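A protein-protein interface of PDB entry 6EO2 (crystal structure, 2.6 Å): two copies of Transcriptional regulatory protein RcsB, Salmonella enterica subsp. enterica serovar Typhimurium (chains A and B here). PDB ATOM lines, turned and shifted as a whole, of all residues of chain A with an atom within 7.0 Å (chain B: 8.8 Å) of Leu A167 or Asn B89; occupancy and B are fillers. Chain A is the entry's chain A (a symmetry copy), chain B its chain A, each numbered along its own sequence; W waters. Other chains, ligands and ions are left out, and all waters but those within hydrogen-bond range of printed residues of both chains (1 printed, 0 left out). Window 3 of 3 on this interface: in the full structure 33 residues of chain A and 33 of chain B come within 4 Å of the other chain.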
ATOM      1  N   LEU A 161     -11.453 -18.815 -28.760  1.00  0.00           N
ATOM      2  CA  LEU A 161     -11.638 -18.369 -27.385  1.00  0.00           C
ATOM      3  C   LEU A 161     -10.381 -17.737 -26.833  1.00  0.00           C
ATOM      4  O   LEU A 161     -10.452 -16.739 -26.117  1.00  0.00           O
ATOM      5  CB  LEU A 161     -12.075 -19.530 -26.490  1.00  0.00           C
ATOM      6  CG  LEU A 161     -13.474 -20.059 -26.799  1.00  0.00           C
ATOM      7  CD1 LEU A 161     -13.778 -21.328 -26.017  1.00  0.00           C
ATOM      8  CD2 LEU A 161     -14.513 -18.982 -26.523  1.00  0.00           C
ATOM      9  N   PHE A 162      -9.225 -18.303 -27.147  1.00  0.00           N
ATOM     10  CA  PHE A 162      -7.987 -17.660 -26.730  1.00  0.00           C
ATOM     11  C   PHE A 162      -7.953 -16.219 -27.246  1.00  0.00           C
ATOM     12  O   PHE A 162      -7.723 -15.291 -26.479  1.00  0.00           O
ATOM     13  CB  PHE A 162      -6.759 -18.423 -27.215  1.00  0.00           C
ATOM     14  CG  PHE A 162      -5.502 -18.045 -26.488  1.00  0.00           C
ATOM     15  CD1 PHE A 162      -5.327 -18.403 -25.158  1.00  0.00           C
ATOM     16  CD2 PHE A 162      -4.493 -17.332 -27.128  1.00  0.00           C
ATOM     17  CE1 PHE A 162      -4.170 -18.058 -24.477  1.00  0.00           C
ATOM     18  CE2 PHE A 162      -3.334 -16.982 -26.455  1.00  0.00           C
ATOM     19  CZ  PHE A 162      -3.171 -17.345 -25.126  1.00  0.00           C
ATOM     20  N   GLU A 164     -10.363 -14.334 -28.075  1.00  0.00           N
ATOM     21  CA  GLU A 164     -11.375 -13.549 -27.357  1.00  0.00           C
ATOM     22  C   GLU A 164     -10.962 -13.189 -25.926  1.00  0.00           C
ATOM     23  O   GLU A 164     -11.704 -12.482 -25.250  1.00  0.00           O
ATOM     24  CB  GLU A 164     -12.720 -14.292 -27.309  1.00  0.00           C
ATOM     25  CG  GLU A 164     -13.404 -14.493 -28.647  1.00  0.00           C
ATOM     26  CD  GLU A 164     -14.101 -13.252 -29.185  1.00  0.00           C
ATOM     27  OE1 GLU A 164     -15.089 -13.413 -29.943  1.00  0.00           O
ATOM     28  OE2 GLU A 164     -13.669 -12.122 -28.869  1.00  0.00           O
ATOM     29  N   GLY A 165      -9.815 -13.687 -25.457  1.00  0.00           N
ATOM     30  CA  GLY A 165      -9.266 -13.310 -24.147  1.00  0.00           C
ATOM     31  C   GLY A 165      -9.446 -14.327 -23.028  1.00  0.00           C
ATOM     32  O   GLY A 165      -9.147 -14.034 -21.870  1.00  0.00           O
ATOM     33  N   PHE A 166      -9.913 -15.527 -23.360  1.00  0.00           N
ATOM     34  CA  PHE A 166     -10.021 -16.609 -22.380  1.00  0.00           C
ATOM     35  C   PHE A 166      -8.647 -17.243 -22.140  1.00  0.00           C
ATOM     36  O   PHE A 166      -7.910 -17.512 -23.088  1.00  0.00           O
ATOM     37  CB  PHE A 166     -10.968 -17.708 -22.877  1.00  0.00           C
ATOM     38  CG  PHE A 166     -12.433 -17.352 -22.802  1.00  0.00           C
ATOM     39  CD1 PHE A 166     -12.947 -16.288 -23.523  1.00  0.00           C
ATOM     40  CD2 PHE A 166     -13.306 -18.117 -22.040  1.00  0.00           C
ATOM     41  CE1 PHE A 166     -14.293 -15.978 -23.469  1.00  0.00           C
ATOM     42  CE2 PHE A 166     -14.658 -17.812 -21.985  1.00  0.00           C
ATOM     43  CZ  PHE A 166     -15.154 -16.741 -22.698  1.00  0.00           C
ATOM     44  N   LEU A 167      -8.307 -17.484 -20.876  1.00  0.00           N
ATOM     45  CA  LEU A 167      -7.145 -18.305 -20.539  1.00  0.00           C
ATOM     46  C   LEU A 167      -7.529 -19.772 -20.717  1.00  0.00           C
ATOM     47  O   LEU A 167      -8.715 -20.107 -20.753  1.00  0.00           O
ATOM     48  CB  LEU A 167      -6.702 -18.043 -19.103  1.00  0.00           C
ATOM     49  CG  LEU A 167      -6.298 -16.607 -18.765  1.00  0.00           C
ATOM     50  CD1 LEU A 167      -6.381 -16.373 -17.267  1.00  0.00           C
ATOM     51  CD2 LEU A 167      -4.899 -16.285 -19.278  1.00  0.00           C
ATOM     52  N   VAL A 168      -6.533 -20.649 -20.828  1.00  0.00           N
ATOM     53  CA  VAL A 168      -6.788 -22.077 -21.081  1.00  0.00           C
ATOM     54  C   VAL A 168      -7.750 -22.709 -20.067  1.00  0.00           C
ATOM     55  O   VAL A 168      -8.602 -23.519 -20.438  1.00  0.00           O
ATOM     56  CB  VAL A 168      -5.473 -22.890 -21.112  1.00  0.00           C
ATOM     57  CG1 VAL A 168      -5.743 -24.387 -21.015  1.00  0.00           C
ATOM     58  CG2 VAL A 168      -4.681 -22.574 -22.378  1.00  0.00           C
ATOM     59  N   THR A 169      -7.624 -22.347 -18.793  1.00  0.00           N
ATOM     60  CA  THR A 169      -8.472 -22.954 -17.766  1.00  0.00           C
ATOM     61  C   THR A 169      -9.938 -22.555 -17.980  1.00  0.00           C
ATOM     62  O   THR A 169     -10.843 -23.378 -17.801  1.00  0.00           O
ATOM     63  CB  THR A 169      -8.000 -22.614 -16.332  1.00  0.00           C
ATOM     64  OG1 THR A 169      -8.093 -21.206 -16.098  1.00  0.00           O
ATOM     65  CG2 THR A 169      -6.547 -23.075 -16.119  1.00  0.00           C
ATOM     66  N   GLU A 170     -10.154 -21.307 -18.396  1.00  0.00           N
ATOM     67  CA  GLU A 170     -11.488 -20.810 -18.733  1.00  0.00           C
ATOM     68  C   GLU A 170     -12.070 -21.505 -19.970  1.00  0.00           C
ATOM     69  O   GLU A 170     -13.283 -21.720 -20.059  1.00  0.00           O
ATOM     70  CB  GLU A 170     -11.448 -19.295 -18.955  1.00  0.00           C
ATOM     71  CG  GLU A 170     -11.111 -18.491 -17.702  1.00  0.00           C
ATOM     72  CD  GLU A 170     -10.551 -17.100 -17.983  1.00  0.00           C
ATOM     73  OE1 GLU A 170     -10.319 -16.749 -19.155  1.00  0.00           O
ATOM     74  OE2 GLU A 170     -10.320 -16.346 -17.014  1.00  0.00           O
ATOM     75  N   ILE A 171     -11.207 -21.858 -20.920  1.00  0.00           N
ATOM     76  CA  ILE A 171     -11.647 -22.550 -22.123  1.00  0.00           C
ATOM     77  C   ILE A 171     -12.096 -23.966 -21.790  1.00  0.00           C
ATOM     78  O   ILE A 171     -13.086 -24.447 -22.346  1.00  0.00           O
ATOM     79  CB  ILE A 171     -10.538 -22.592 -23.200  1.00  0.00           C
ATOM     80  CG1 ILE A 171     -10.204 -21.166 -23.666  1.00  0.00           C
ATOM     81  CG2 ILE A 171     -10.966 -23.456 -24.387  1.00  0.00           C
ATOM     82  CD1 ILE A 171      -9.078 -21.075 -24.674  1.00  0.00           C
ATOM     83  N   ALA A 172     -11.358 -24.634 -20.903  1.00  0.00           N
ATOM     84  CA  ALA A 172     -11.709 -25.991 -20.453  1.00  0.00           C
ATOM     85  C   ALA A 172     -13.122 -26.036 -19.859  1.00  0.00           C
ATOM     86  O   ALA A 172     -13.905 -26.937 -20.145  1.00  0.00           O
ATOM     87  CB  ALA A 172     -10.698 -26.473 -19.427  1.00  0.00           C
ATOM     88  N   ILE A 182      -7.185 -29.406 -23.572  1.00  0.00           N
ATOM     89  CA  ILE A 182      -7.183 -28.074 -24.172  1.00  0.00           C
ATOM     90  C   ILE A 182      -5.766 -27.648 -24.546  1.00  0.00           C
ATOM     91  O   ILE A 182      -5.521 -27.247 -25.677  1.00  0.00           O
ATOM     92  CB  ILE A 182      -7.830 -27.013 -23.246  1.00  0.00           C
ATOM     93  CG1 ILE A 182      -9.306 -27.346 -22.965  1.00  0.00           C
ATOM     94  CG2 ILE A 182      -7.721 -25.619 -23.863  1.00  0.00           C
ATOM     95  CD1 ILE A 182     -10.176 -27.471 -24.199  1.00  0.00           C
ATOM     96  N   LEU A 202      -1.456 -14.618 -31.189  1.00  0.00           N
ATOM     97  CA  LEU A 202      -2.472 -13.575 -31.131  1.00  0.00           C
ATOM     98  C   LEU A 202      -2.268 -12.547 -32.246  1.00  0.00           C
ATOM     99  O   LEU A 202      -3.238 -12.079 -32.846  1.00  0.00           O
ATOM    100  CB  LEU A 202      -2.490 -12.919 -29.750  1.00  0.00           C
ATOM    101  CG  LEU A 202      -3.007 -13.831 -28.635  1.00  0.00           C
ATOM    102  CD1 LEU A 202      -2.819 -13.183 -27.270  1.00  0.00           C
ATOM    103  CD2 LEU A 202      -4.464 -14.201 -28.853  1.00  0.00           C
ATOM    104  N   ASP B  56     -16.408  -9.181 -16.078  1.00  0.00           N
ATOM    105  CA  ASP B  56     -15.289 -10.061 -16.369  1.00  0.00           C
ATOM    106  C   ASP B  56     -15.090 -10.089 -17.869  1.00  0.00           C
ATOM    107  O   ASP B  56     -16.052 -10.006 -18.636  1.00  0.00           O
ATOM    108  CB  ASP B  56     -15.585 -11.475 -15.852  1.00  0.00           C
ATOM    109  CG  ASP B  56     -14.369 -12.408 -15.904  1.00  0.00           C
ATOM    110  OD1 ASP B  56     -13.214 -11.954 -16.144  1.00  0.00           O
ATOM    111  OD2 ASP B  56     -14.598 -13.626 -15.702  1.00  0.00           O
ATOM    112  N   LEU B  57     -13.841 -10.203 -18.291  1.00  0.00           N
ATOM    113  CA  LEU B  57     -13.539 -10.311 -19.706  1.00  0.00           C
ATOM    114  C   LEU B  57     -14.009 -11.657 -20.226  1.00  0.00           C
ATOM    115  O   LEU B  57     -14.648 -11.744 -21.256  1.00  0.00           O
ATOM    116  CB  LEU B  57     -12.040 -10.166 -19.924  1.00  0.00           C
ATOM    117  CG  LEU B  57     -11.541 -10.242 -21.359  1.00  0.00           C
ATOM    118  CD1 LEU B  57     -12.396  -9.395 -22.290  1.00  0.00           C
ATOM    119  CD2 LEU B  57     -10.089  -9.796 -21.385  1.00  0.00           C
ATOM    120  N   SER B  58     -13.718 -12.701 -19.466  1.00  0.00           N
ATOM    121  CA  SER B  58     -13.948 -14.067 -19.889  1.00  0.00           C
ATOM    122  C   SER B  58     -15.260 -14.664 -19.369  1.00  0.00           C
ATOM    123  O   SER B  58     -15.273 -15.790 -18.881  1.00  0.00           O
ATOM    124  CB  SER B  58     -12.784 -14.913 -19.381  1.00  0.00           C
ATOM    125  OG  SER B  58     -12.872 -15.078 -17.976  1.00  0.00           O
ATOM    126  N   ILE B  68     -13.950 -10.477 -25.628  1.00  0.00           N
ATOM    127  CA  ILE B  68     -13.863  -9.136 -26.198  1.00  0.00           C
ATOM    128  C   ILE B  68     -15.074  -8.810 -27.060  1.00  0.00           C
ATOM    129  O   ILE B  68     -15.561  -7.681 -27.060  1.00  0.00           O
ATOM    130  CB  ILE B  68     -12.567  -8.997 -27.015  1.00  0.00           C
ATOM    131  CG1 ILE B  68     -11.375  -8.930 -26.058  1.00  0.00           C
ATOM    132  CG2 ILE B  68     -12.593  -7.762 -27.903  1.00  0.00           C
ATOM    133  CD1 ILE B  68     -10.032  -8.995 -26.751  1.00  0.00           C
ATOM    134  N   VAL B  85     -13.616  -3.163 -17.111  1.00  0.00           N
ATOM    135  CA  VAL B  85     -13.341  -4.565 -17.413  1.00  0.00           C
ATOM    136  C   VAL B  85     -12.418  -5.145 -16.366  1.00  0.00           C
ATOM    137  O   VAL B  85     -11.310  -4.655 -16.159  1.00  0.00           O
ATOM    138  CB  VAL B  85     -12.725  -4.734 -18.817  1.00  0.00           C
ATOM    139  CG1 VAL B  85     -11.978  -6.060 -18.949  1.00  0.00           C
ATOM    140  CG2 VAL B  85     -13.819  -4.643 -19.872  1.00  0.00           C
ATOM    141  N   LEU B  86     -12.884  -6.204 -15.722  1.00  0.00           N
ATOM    142  CA  LEU B  86     -12.139  -6.867 -14.665  1.00  0.00           C
ATOM    143  C   LEU B  86     -11.598  -8.176 -15.227  1.00  0.00           C
ATOM    144  O   LEU B  86     -12.366  -8.986 -15.733  1.00  0.00           O
ATOM    145  CB  LEU B  86     -13.084  -7.118 -13.491  1.00  0.00           C
ATOM    146  CG  LEU B  86     -12.543  -7.458 -12.101  1.00  0.00           C
ATOM    147  CD1 LEU B  86     -11.334  -6.627 -11.702  1.00  0.00           C
ATOM    148  CD2 LEU B  86     -13.665  -7.277 -11.086  1.00  0.00           C
ATOM    149  N   THR B  87     -10.288  -8.385 -15.180  1.00  0.00           N
ATOM    150  CA  THR B  87      -9.743  -9.627 -15.713  1.00  0.00           C
ATOM    151  C   THR B  87      -8.491 -10.092 -15.012  1.00  0.00           C
ATOM    152  O   THR B  87      -7.818  -9.336 -14.318  1.00  0.00           O
ATOM    153  CB  THR B  87      -9.456  -9.532 -17.226  1.00  0.00           C
ATOM    154  OG1 THR B  87      -9.090 -10.823 -17.732  1.00  0.00           O
ATOM    155  CG2 THR B  87      -8.338  -8.540 -17.522  1.00  0.00           C
ATOM    156  N   MET B  88      -8.204 -11.369 -15.207  1.00  0.00           N
ATOM    157  CA  MET B  88      -7.005 -11.992 -14.695  1.00  0.00           C
ATOM    158  C   MET B  88      -6.003 -12.263 -15.821  1.00  0.00           C
ATOM    159  O   MET B  88      -4.902 -12.754 -15.575  1.00  0.00           O
ATOM    160  CB  MET B  88      -7.392 -13.295 -14.018  1.00  0.00           C
ATOM    161  CG  MET B  88      -6.470 -13.684 -12.886  1.00  0.00           C
ATOM    162  SD  MET B  88      -7.260 -14.842 -11.764  1.00  0.00           S
ATOM    163  CE  MET B  88      -7.971 -16.028 -12.910  1.00  0.00           C
ATOM    164  N   ASN B  89      -6.386 -11.946 -17.056  1.00  0.00           N
ATOM    165  CA  ASN B  89      -5.533 -12.182 -18.205  1.00  0.00           C
ATOM    166  C   ASN B  89      -4.548 -11.038 -18.346  1.00  0.00           C
ATOM    167  O   ASN B  89      -4.927  -9.920 -18.702  1.00  0.00           O
ATOM    168  CB  ASN B  89      -6.369 -12.316 -19.480  1.00  0.00           C
ATOM    169  CG  ASN B  89      -5.585 -12.917 -20.628  1.00  0.00           C
ATOM    170  OD1 ASN B  89      -4.362 -12.826 -20.675  1.00  0.00           O
ATOM    171  ND2 ASN B  89      -6.290 -13.541 -21.557  1.00  0.00           N
ATOM    172  N   ASN B  90      -3.281 -11.324 -18.065  1.00  0.00           N
ATOM    173  CA  ASN B  90      -2.234 -10.307 -18.143  1.00  0.00           C
ATOM    174  C   ASN B  90      -1.372 -10.429 -19.408  1.00  0.00           C
ATOM    175  O   ASN B  90      -0.248  -9.935 -19.453  1.00  0.00           O
ATOM    176  CB  ASN B  90      -1.378 -10.304 -16.867  1.00  0.00           C
ATOM    177  CG  ASN B  90      -0.688 -11.627 -16.610  1.00  0.00           C
ATOM    178  OD1 ASN B  90      -0.819 -12.587 -17.382  1.00  0.00           O
ATOM    179  ND2 ASN B  90       0.052 -11.688 -15.510  1.00  0.00           N
ATOM    180  N   ASN B  91      -1.916 -11.088 -20.430  1.00  0.00           N
ATOM    181  CA  ASN B  91      -1.334 -11.070 -21.764  1.00  0.00           C
ATOM    182  C   ASN B  91      -1.477  -9.659 -22.377  1.00  0.00           C
ATOM    183  O   ASN B  91      -2.585  -9.116 -22.422  1.00  0.00           O
ATOM    184  CB  ASN B  91      -2.034 -12.109 -22.638  1.00  0.00           C
ATOM    185  CG  ASN B  91      -1.364 -12.295 -23.976  1.00  0.00           C
ATOM    186  OD1 ASN B  91      -1.049 -11.331 -24.665  1.00  0.00           O
ATOM    187  ND2 ASN B  91      -1.159 -13.541 -24.363  1.00  0.00           N
ATOM    188  N   PRO B  92      -0.363  -9.064 -22.849  1.00  0.00           N
ATOM    189  CA  PRO B  92      -0.378  -7.689 -23.367  1.00  0.00           C
ATOM    190  C   PRO B  92      -1.246  -7.478 -24.608  1.00  0.00           C
ATOM    191  O   PRO B  92      -1.934  -6.461 -24.713  1.00  0.00           O
ATOM    192  CB  PRO B  92       1.090  -7.425 -23.718  1.00  0.00           C
ATOM    193  CG  PRO B  92       1.868  -8.426 -22.939  1.00  0.00           C
ATOM    194  CD  PRO B  92       0.996  -9.636 -22.873  1.00  0.00           C
ATOM    195  N   ALA B  93      -1.192  -8.421 -25.542  1.00  0.00           N
ATOM    196  CA  ALA B  93      -2.038  -8.382 -26.742  1.00  0.00           C
ATOM    197  C   ALA B  93      -3.534  -8.361 -26.410  1.00  0.00           C
ATOM    198  O   ALA B  93      -4.329  -7.729 -27.117  1.00  0.00           O
ATOM    199  CB  ALA B  93      -1.725  -9.574 -27.638  1.00  0.00           C
ATOM    200  N   ILE B  94      -3.908  -9.068 -25.346  1.00  0.00           N
ATOM    201  CA  ILE B  94      -5.296  -9.124 -24.898  1.00  0.00           C
ATOM    202  C   ILE B  94      -5.691  -7.797 -24.248  1.00  0.00           C
ATOM    203  O   ILE B  94      -6.727  -7.217 -24.573  1.00  0.00           O
ATOM    204  CB  ILE B  94      -5.518 -10.308 -23.922  1.00  0.00           C
ATOM    205  CG1 ILE B  94      -5.351 -11.644 -24.660  1.00  0.00           C
ATOM    206  CG2 ILE B  94      -6.886 -10.225 -23.234  1.00  0.00           C
ATOM    207  CD1 ILE B  94      -6.328 -11.868 -25.799  1.00  0.00           C
ATOM    208  N   LEU B  95      -4.856  -7.307 -23.344  1.00  0.00           N
ATOM    209  CA  LEU B  95      -5.130  -6.034 -22.678  1.00  0.00           C
ATOM    210  C   LEU B  95      -5.176  -4.878 -23.677  1.00  0.00           C
ATOM    211  O   LEU B  95      -5.952  -3.935 -23.512  1.00  0.00           O
ATOM    212  CB  LEU B  95      -4.069  -5.748 -21.617  1.00  0.00           C
ATOM    213  CG  LEU B  95      -3.988  -6.766 -20.481  1.00  0.00           C
ATOM    214  CD1 LEU B  95      -2.698  -6.585 -19.689  1.00  0.00           C
ATOM    215  CD2 LEU B  95      -5.213  -6.682 -19.580  1.00  0.00           C
ATOM    216  N   SER B  96      -4.347  -4.957 -24.709  1.00  0.00           N
ATOM    217  CA  SER B  96      -4.307  -3.927 -25.730  1.00  0.00           C
ATOM    218  C   SER B  96      -5.589  -3.938 -26.574  1.00  0.00           C
ATOM    219  O   SER B  96      -6.220  -2.897 -26.784  1.00  0.00           O
ATOM    220  CB  SER B  96      -3.083  -4.129 -26.616  1.00  0.00           C
ATOM    221  OG  SER B  96      -3.073  -3.173 -27.653  1.00  0.00           O
ATOM    222  N   VAL B  98      -8.407  -4.936 -25.723  1.00  0.00           N
ATOM    223  CA  VAL B  98      -9.468  -4.453 -24.844  1.00  0.00           C
ATOM    224  C   VAL B  98      -9.501  -2.932 -24.846  1.00  0.00           C
ATOM    225  O   VAL B  98     -10.559  -2.335 -25.042  1.00  0.00           O
ATOM    226  CB  VAL B  98      -9.298  -4.974 -23.390  1.00  0.00           C
ATOM    227  CG1 VAL B  98     -10.282  -4.299 -22.446  1.00  0.00           C
ATOM    228  CG2 VAL B  98      -9.481  -6.485 -23.326  1.00  0.00           C
ATOM    229  N   ILE B 106      -9.621  -0.498 -17.045  1.00  0.00           N
ATOM    230  CA  ILE B 106      -9.292  -1.909 -16.817  1.00  0.00           C
ATOM    231  C   ILE B 106      -8.704  -2.100 -15.421  1.00  0.00           C
ATOM    232  O   ILE B 106      -7.918  -1.282 -14.947  1.00  0.00           O
ATOM    233  CB  ILE B 106      -8.267  -2.453 -17.832  1.00  0.00           C
ATOM    234  CG1 ILE B 106      -8.862  -2.452 -19.231  1.00  0.00           C
ATOM    235  CG2 ILE B 106      -7.839  -3.875 -17.465  1.00  0.00           C
ATOM    236  CD1 ILE B 106      -7.939  -3.033 -20.283  1.00  0.00           C
ATOM    237  N   VAL B 107      -9.087  -3.199 -14.784  1.00  0.00           N
ATOM    238  CA  VAL B 107      -8.558  -3.581 -13.492  1.00  0.00           C
ATOM    239  C   VAL B 107      -8.176  -5.054 -13.569  1.00  0.00           C
ATOM    240  O   VAL B 107      -8.947  -5.865 -14.070  1.00  0.00           O
ATOM    241  CB  VAL B 107      -9.618  -3.375 -12.391  1.00  0.00           C
ATOM    242  CG1 VAL B 107      -9.094  -3.849 -11.040  1.00  0.00           C
ATOM    243  CG2 VAL B 107     -10.060  -1.916 -12.329  1.00  0.00           C
ATOM    244  N   LEU B 108      -6.983  -5.401 -13.100  1.00  0.00           N
ATOM    245  CA  LEU B 108      -6.598  -6.810 -13.001  1.00  0.00           C
ATOM    246  C   LEU B 108      -7.091  -7.349 -11.665  1.00  0.00           C
ATOM    247  O   LEU B 108      -7.089  -6.634 -10.667  1.00  0.00           O
ATOM    248  CB  LEU B 108      -5.085  -6.979 -13.126  1.00  0.00           C
ATOM    249  CG  LEU B 108      -4.504  -6.607 -14.489  1.00  0.00           C
ATOM    250  CD1 LEU B 108      -2.992  -6.528 -14.409  1.00  0.00           C
ATOM    251  CD2 LEU B 108      -4.925  -7.612 -15.548  1.00  0.00           C
ATOM    252  N   LYS B 109      -7.523  -8.603 -11.643  1.00  0.00           N
ATOM    253  CA  LYS B 109      -8.058  -9.190 -10.415  1.00  0.00           C
ATOM    254  C   LYS B 109      -6.945  -9.438  -9.394  1.00  0.00           C
ATOM    255  O   LYS B 109      -7.128  -9.201  -8.209  1.00  0.00           O
ATOM    256  CB  LYS B 109      -8.806 -10.480 -10.727  1.00  0.00           C
ATOM    257  CG  LYS B 109     -10.049 -10.268 -11.572  1.00  0.00           C
ATOM    258  CD  LYS B 109     -10.680 -11.592 -11.980  1.00  0.00           C
ATOM    259  CE  LYS B 109     -12.027 -11.362 -12.640  1.00  0.00           C
ATOM    260  NZ  LYS B 109     -12.732 -12.622 -12.990  1.00  0.00           N
ATOM    261  N   GLN B 110      -5.793  -9.894  -9.882  1.00  0.00           N
ATOM    262  CA  GLN B 110      -4.590 -10.103  -9.058  1.00  0.00           C
ATOM    263  C   GLN B 110      -3.761  -8.830  -8.851  1.00  0.00           C
ATOM    264  O   GLN B 110      -2.710  -8.862  -8.203  1.00  0.00           O
ATOM    265  CB  GLN B 110      -3.694 -11.197  -9.660  1.00  0.00           C
ATOM    266  CG  GLN B 110      -3.038 -10.867 -10.991  1.00  0.00           C
ATOM    267  CD  GLN B 110      -3.974 -11.077 -12.159  1.00  0.00           C
ATOM    268  OE1 GLN B 110      -4.963 -10.358 -12.310  1.00  0.00           O
ATOM    269  NE2 GLN B 110      -3.674 -12.064 -12.989  1.00  0.00           N
ATOM    270  N   SER B 133       0.341  -1.545 -12.991  1.00  0.00           N
ATOM    271  CA  SER B 133       0.571  -2.961 -13.307  1.00  0.00           C
ATOM    272  C   SER B 133       0.147  -3.301 -14.741  1.00  0.00           C
ATOM    273  O   SER B 133       0.710  -4.203 -15.359  1.00  0.00           O
ATOM    274  CB  SER B 133      -0.150  -3.873 -12.302  1.00  0.00           C
ATOM    275  OG  SER B 133      -1.537  -3.590 -12.234  1.00  0.00           O
ATOM    276  N   VAL B 134      -0.846  -2.577 -15.258  1.00  0.00           N
ATOM    277  CA  VAL B 134      -1.232  -2.660 -16.665  1.00  0.00           C
ATOM    278  C   VAL B 134      -0.317  -1.792 -17.537  1.00  0.00           C
ATOM    279  O   VAL B 134       0.125  -2.231 -18.592  1.00  0.00           O
ATOM    280  CB  VAL B 134      -2.707  -2.237 -16.870  1.00  0.00           C
ATOM    281  CG1 VAL B 134      -3.065  -2.153 -18.348  1.00  0.00           C
ATOM    282  CG2 VAL B 134      -3.642  -3.202 -16.158  1.00  0.00           C
ATOM    283  N   LEU B 137       3.122  -3.505 -18.221  1.00  0.00           N
ATOM    284  CA  LEU B 137       2.945  -4.677 -19.092  1.00  0.00           C
ATOM    285  C   LEU B 137       2.749  -4.296 -20.565  1.00  0.00           C
ATOM    286  O   LEU B 137       3.024  -5.103 -21.453  1.00  0.00           O
ATOM    287  CB  LEU B 137       1.767  -5.549 -18.632  1.00  0.00           C
ATOM    288  CG  LEU B 137       2.037  -6.560 -17.512  1.00  0.00           C
ATOM    289  CD1 LEU B 137       0.734  -7.151 -16.989  1.00  0.00           C
ATOM    290  CD2 LEU B 137       2.973  -7.664 -17.983  1.00  0.00           C
HETATM  291  O   HOH W   1      -6.296 -15.378 -23.970  1.00  0.00           O
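Printed residues of chain A that touch a printed residue of chain B: Phe A162, Glu A164, Gly A165, Phe A166, Leu A167, Glu A170 and Leu A202. Hydrophobic or aromatic side chains of chain B within 4 Å of the printed part of chain A: Ile B68, Ala B93 and Ile B94. Along chain B the printed residues that touch a printed residue of chain A span positions 58 to 94. Among the printed residues, 10 pairs touch across the chains. Among the printed residues, no Asp or Glu carboxylate lies within 4 Å of a Lys or Arg side-chain nitrogen of the other chain.
The backbone carbonyl oxygen of Leu A161 is in hydrogen-bond range of the backbone NH of Phe A166 (3.1 Å). The backbone NH (N) of Leu A167 lies within hydrogen-bond range of the side-chain carboxylate (OE1) of Glu A170 (2.7 Å). OD2 of Asp B56 sits at hydrogen-bond distance from OG of Ser B58, at 3.2 Å. The side-chain amide oxygen (OD1) of Asn B89 sits at hydrogen-bond distance from the backbone NH (N) of Asn B91 (3.0 Å). The backbone NH (N) of Ala B93 sits at hydrogen-bond distance from the side-chain amide oxygen (OD1) of Asn B91 (3.0 Å). OG1 of Thr B87 lies within hydrogen-bond range of N of Asn B89, at 3.0 Å.
Phe A162 touches Ile B94. Gly A165 touches Ile B94 (CA to CD1, 3.7 Å). Phe A166 touches Ser B58 (CE2 to O, 3.8 Å). Leu A167 touches Asn B89 (CD2 to CG, 3.7 Å). Asn B91 touches Leu A202. CB of Ala B93 touches CD1 of Leu A202, at 3.8 Å. Ile B94 touches Leu A202.
The side-chain amide nitrogen (ND2) of Asn B89 lies within hydrogen-bond range of the backbone carbonyl oxygen (O) of Gly A165, 2.9 Å away. The side-chain carboxylate of Glu A170 sits at hydrogen-bond distance from the side-chain hydroxyl of Ser B58 (3.0 Å). The backbone NH of Ile B68 sits at hydrogen-bond distance from the backbone carbonyl oxygen of Glu A164 (3.0 Å).
No position is printed for both chains. Of the 10 pairs that touch across the chains among the printed residues, none has its exchanged pair printed and touching as well.
Printed residues of chain B within 4 Å of Phe A166: Ser B58. Leu A167 touches one residue of chain B. Ile A182 touches none of the printed residues of chain B. Of the printed residues of chain A, Asn B91 touches Leu A202. Of the printed residues of chain A, Ala B93 touches Leu A202 (3.8 Å). Of the printed residues of chain A, Ile B94 touches Phe A162, Gly A165 and Leu A202. Leu B137 touches none of the printed residues of chain A. The nearest residue of chain A that does not touch Asn B89 is Phe A166 (4.4 Å). The nearest printed residue of chain A that does not touch Asn B91 is Phe A162 (4.4 Å).
Water W1 lies within hydrogen-bond range of O of Phe A166 (2.8 Å), O of Phe A162 (2.9 Å) and ND2 of Asn B89 (3.0 Å).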
